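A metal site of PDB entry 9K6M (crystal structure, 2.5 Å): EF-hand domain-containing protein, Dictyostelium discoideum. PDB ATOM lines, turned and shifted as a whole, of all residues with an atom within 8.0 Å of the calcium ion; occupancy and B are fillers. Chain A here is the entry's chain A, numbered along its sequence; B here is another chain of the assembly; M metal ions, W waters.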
ATOM      1  N   PHE A 131      13.543  25.710  -6.733  1.00  0.00           N
ATOM      2  CA  PHE A 131      12.094  25.740  -6.802  1.00  0.00           C
ATOM      3  C   PHE A 131      11.553  26.780  -5.815  1.00  0.00           C
ATOM      4  O   PHE A 131      10.747  27.613  -6.192  1.00  0.00           O
ATOM      5  CB  PHE A 131      11.541  24.330  -6.567  1.00  0.00           C
ATOM      6  CG  PHE A 131      10.053  24.211  -6.746  1.00  0.00           C
ATOM      7  CD1 PHE A 131       9.499  24.094  -8.013  1.00  0.00           C
ATOM      8  CD2 PHE A 131       9.205  24.205  -5.659  1.00  0.00           C
ATOM      9  CE1 PHE A 131       8.132  23.984  -8.172  1.00  0.00           C
ATOM     10  CE2 PHE A 131       7.838  24.116  -5.815  1.00  0.00           C
ATOM     11  CZ  PHE A 131       7.299  24.017  -7.075  1.00  0.00           C
ATOM     12  N   MET A 134      11.872  30.362  -6.936  1.00  0.00           N
ATOM     13  CA  MET A 134      11.104  30.800  -8.091  1.00  0.00           C
ATOM     14  C   MET A 134       9.616  30.655  -7.802  1.00  0.00           C
ATOM     15  O   MET A 134       8.797  31.192  -8.529  1.00  0.00           O
ATOM     16  CB  MET A 134      11.525  30.011  -9.337  1.00  0.00           C
ATOM     17  CG  MET A 134      13.025  30.220  -9.699  1.00  0.00           C
ATOM     18  SD  MET A 134      13.773  29.175 -11.010  1.00  0.00           S
ATOM     19  CE  MET A 134      12.342  28.276 -11.591  1.00  0.00           C
ATOM     20  N   ASP A 135       9.245  30.003  -6.698  1.00  0.00           N
ATOM     21  CA  ASP A 135       7.844  29.890  -6.297  1.00  0.00           C
ATOM     22  C   ASP A 135       7.466  31.119  -5.467  1.00  0.00           C
ATOM     23  O   ASP A 135       7.440  31.058  -4.241  1.00  0.00           O
ATOM     24  CB  ASP A 135       7.585  28.626  -5.478  1.00  0.00           C
ATOM     25  CG  ASP A 135       6.181  28.550  -4.933  1.00  0.00           C
ATOM     26  OD1 ASP A 135       5.295  29.201  -5.536  1.00  0.00           O
ATOM     27  OD2 ASP A 135       5.975  27.865  -3.905  1.00  0.00           O
ATOM     28  N   VAL A 136       7.180  32.231  -6.123  1.00  0.00           N
ATOM     29  CA  VAL A 136       7.259  33.520  -5.456  1.00  0.00           C
ATOM     30  C   VAL A 136       6.124  33.657  -4.438  1.00  0.00           C
ATOM     31  O   VAL A 136       6.344  34.240  -3.390  1.00  0.00           O
ATOM     32  CB  VAL A 136       7.323  34.695  -6.460  1.00  0.00           C
ATOM     33  CG1 VAL A 136       6.093  34.756  -7.337  1.00  0.00           C
ATOM     34  CG2 VAL A 136       7.524  36.030  -5.779  1.00  0.00           C
ATOM     35  N   ASN A 137       4.952  33.041  -4.675  1.00  0.00           N
ATOM     36  CA  ASN A 137       3.850  33.220  -3.740  1.00  0.00           C
ATOM     37  C   ASN A 137       3.730  32.054  -2.746  1.00  0.00           C
ATOM     38  O   ASN A 137       2.734  31.998  -2.007  1.00  0.00           O
ATOM     39  CB  ASN A 137       2.526  33.360  -4.497  1.00  0.00           C
ATOM     40  CG  ASN A 137       2.115  32.078  -5.169  1.00  0.00           C
ATOM     41  OD1 ASN A 137       2.842  31.079  -5.104  1.00  0.00           O
ATOM     42  ND2 ASN A 137       0.941  32.084  -5.773  1.00  0.00           N
ATOM     43  N   GLY A 138       4.713  31.122  -2.737  1.00  0.00           N
ATOM     44  CA  GLY A 138       4.821  30.052  -1.753  1.00  0.00           C
ATOM     45  C   GLY A 138       3.679  29.006  -1.749  1.00  0.00           C
ATOM     46  O   GLY A 138       3.530  28.276  -0.780  1.00  0.00           O
ATOM     47  N   ASP A 139       2.916  28.845  -2.836  1.00  0.00           N
ATOM     48  CA  ASP A 139       1.802  27.902  -2.853  1.00  0.00           C
ATOM     49  C   ASP A 139       2.268  26.482  -3.212  1.00  0.00           C
ATOM     50  O   ASP A 139       1.442  25.551  -3.249  1.00  0.00           O
ATOM     51  CB  ASP A 139       0.692  28.371  -3.803  1.00  0.00           C
ATOM     52  CG  ASP A 139       1.085  28.541  -5.271  1.00  0.00           C
ATOM     53  OD1 ASP A 139       2.264  28.232  -5.648  1.00  0.00           O
ATOM     54  OD2 ASP A 139       0.205  28.972  -6.053  1.00  0.00           O
ATOM     55  N   GLY A 140       3.569  26.321  -3.532  1.00  0.00           N
ATOM     56  CA  GLY A 140       4.142  25.016  -3.864  1.00  0.00           C
ATOM     57  C   GLY A 140       3.936  24.639  -5.334  1.00  0.00           C
ATOM     58  O   GLY A 140       4.001  23.474  -5.675  1.00  0.00           O
ATOM     59  N   SER A 141       3.635  25.638  -6.179  1.00  0.00           N
ATOM     60  CA  SER A 141       3.535  25.421  -7.616  1.00  0.00           C
ATOM     61  C   SER A 141       4.223  26.560  -8.341  1.00  0.00           C
ATOM     62  O   SER A 141       4.215  27.692  -7.874  1.00  0.00           O
ATOM     63  CB  SER A 141       2.123  25.333  -8.078  1.00  0.00           C
ATOM     64  OG  SER A 141       1.558  24.102  -7.688  1.00  0.00           O
ATOM     65  N   ILE A 142       4.790  26.243  -9.522  1.00  0.00           N
ATOM     66  CA  ILE A 142       5.274  27.281 -10.408  1.00  0.00           C
ATOM     67  C   ILE A 142       4.273  27.469 -11.549  1.00  0.00           C
ATOM     68  O   ILE A 142       4.021  26.540 -12.314  1.00  0.00           O
ATOM     69  CB  ILE A 142       6.701  26.989 -10.887  1.00  0.00           C
ATOM     70  CG1 ILE A 142       7.671  27.163  -9.725  1.00  0.00           C
ATOM     71  CG2 ILE A 142       7.066  27.857 -12.060  1.00  0.00           C
ATOM     72  CD1 ILE A 142       9.111  27.073 -10.121  1.00  0.00           C
ATOM     73  N   ASP A 143       3.725  28.689 -11.623  1.00  0.00           N
ATOM     74  CA  ASP A 143       2.747  29.047 -12.634  1.00  0.00           C
ATOM     75  C   ASP A 143       3.473  29.810 -13.739  1.00  0.00           C
ATOM     76  O   ASP A 143       4.627  30.203 -13.564  1.00  0.00           O
ATOM     77  CB  ASP A 143       1.532  29.784 -12.043  1.00  0.00           C
ATOM     78  CG  ASP A 143       1.809  31.172 -11.481  1.00  0.00           C
ATOM     79  OD1 ASP A 143       2.900  31.697 -11.772  1.00  0.00           O
ATOM     80  OD2 ASP A 143       0.943  31.704 -10.743  1.00  0.00           O
ATOM     81  N   ALA A 144       2.792  29.972 -14.872  1.00  0.00           N
ATOM     82  CA  ALA A 144       3.358  30.576 -16.065  1.00  0.00           C
ATOM     83  C   ALA A 144       3.915  31.973 -15.756  1.00  0.00           C
ATOM     84  O   ALA A 144       4.960  32.381 -16.269  1.00  0.00           O
ATOM     85  CB  ALA A 144       2.305  30.632 -17.126  1.00  0.00           C
ATOM     86  N   GLU A 146       5.004  33.261 -12.867  1.00  0.00           N
ATOM     87  CA  GLU A 146       6.200  33.269 -12.045  1.00  0.00           C
ATOM     88  C   GLU A 146       7.394  33.026 -12.957  1.00  0.00           C
ATOM     89  O   GLU A 146       8.450  33.616 -12.756  1.00  0.00           O
ATOM     90  CB  GLU A 146       6.084  32.248 -10.907  1.00  0.00           C
ATOM     91  CG  GLU A 146       4.996  32.562  -9.898  1.00  0.00           C
ATOM     92  CD  GLU A 146       4.688  31.487  -8.866  1.00  0.00           C
ATOM     93  OE1 GLU A 146       4.593  30.296  -9.270  1.00  0.00           O
ATOM     94  OE2 GLU A 146       4.506  31.825  -7.644  1.00  0.00           O
ATOM     95  N   ARG A 190       0.348  24.217 -14.050  1.00  0.00           N
ATOM     96  CA  ARG A 190       1.411  24.608 -13.145  1.00  0.00           C
ATOM     97  C   ARG A 190       2.338  23.439 -12.874  1.00  0.00           C
ATOM     98  O   ARG A 190       1.978  22.294 -13.108  1.00  0.00           O
ATOM     99  CB  ARG A 190       0.807  25.097 -11.823  1.00  0.00           C
ATOM    100  CG  ARG A 190      -0.067  26.330 -11.988  1.00  0.00           C
ATOM    101  CD  ARG A 190      -0.555  26.918 -10.687  1.00  0.00           C
ATOM    102  NE  ARG A 190      -1.260  25.908  -9.919  1.00  0.00           N
ATOM    103  CZ  ARG A 190      -1.833  26.146  -8.755  1.00  0.00           C
ATOM    104  NH1 ARG A 190      -1.840  27.374  -8.257  1.00  0.00           N
ATOM    105  NH2 ARG A 190      -2.448  25.163  -8.115  1.00  0.00           N
ATOM    106  N   LEU A 191       3.507  23.744 -12.307  1.00  0.00           N
ATOM    107  CA  LEU A 191       4.456  22.701 -11.955  1.00  0.00           C
ATOM    108  C   LEU A 191       4.586  22.570 -10.430  1.00  0.00           C
ATOM    109  O   LEU A 191       4.940  23.507  -9.712  1.00  0.00           O
ATOM    110  CB  LEU A 191       5.802  23.045 -12.598  1.00  0.00           C
ATOM    111  CG  LEU A 191       5.768  23.266 -14.105  1.00  0.00           C
ATOM    112  CD1 LEU A 191       7.076  23.848 -14.599  1.00  0.00           C
ATOM    113  CD2 LEU A 191       5.485  21.962 -14.837  1.00  0.00           C
ATOM    114  N   ASP B 310      -0.693  24.396  -1.526  1.00  0.00           N
ATOM    115  CA  ASP B 310      -1.819  25.011  -0.843  1.00  0.00           C
ATOM    116  C   ASP B 310      -3.096  24.250  -1.197  1.00  0.00           C
ATOM    117  O   ASP B 310      -3.390  24.028  -2.369  1.00  0.00           O
ATOM    118  CB  ASP B 310      -1.915  26.485  -1.227  1.00  0.00           C
ATOM    119  CG  ASP B 310      -0.914  27.396  -0.528  1.00  0.00           C
ATOM    120  OD1 ASP B 310      -0.238  26.935   0.433  1.00  0.00           O
ATOM    121  OD2 ASP B 310      -0.808  28.576  -0.946  1.00  0.00           O
HETATM  122 CA    CA M   1       3.489  29.619  -7.016  1.00  0.00          CA
HETATM  123  O   HOH W   1       1.902  29.759  -8.481  1.00  0.00           O
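Water W1 bridges OD2 of Asp 139 (3.1 Å) and OD2 of Asp 143 (3.1 Å).
Water W1 is bound to the calcium ion, 2.2 Å away. The backbone carbonyl oxygen (O) of Ser 141 binds the calcium ion (2.2 Å). OD1 of Asp 139 is bound to the calcium ion (2.3 Å). OD1 of Asp 135 binds the calcium ion. The calcium ion is bound by OD1 of Asn 137, at 2.5 Å. OE2 of Glu 146 is bound to the calcium ion, at 2.5 Å. The calcium ion is bound by the side-chain carboxylate (OE1) of Glu 146.
The backbone NH (N) of Asp 310 of chain B sits at hydrogen-bond distance from the backbone carbonyl oxygen (O) of Asp 139. The side-chain carboxylate of Asp 135 lies within hydrogen-bond range of the backbone NH of Gly 140, at 2.9 Å. The guanidinium group (NH1) of Arg 190 is in salt-bridge range of the side-chain carboxylate (OD2) of Asp 139 (3.4 Å). OD1 of Asp 135 sits close to N of Gly 138 (3.4 Å). N of Glu 146 sits at hydrogen-bond distance from OD1 of Asp 143 (2.8 Å). OE2 of Glu 146 sits close to N of Val 136 (3.1 Å).
Five residues have an atom within 4 Å of the calcium ion: Asp 135, Asn 137, Asp 139, Ser 141 and Glu 146.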
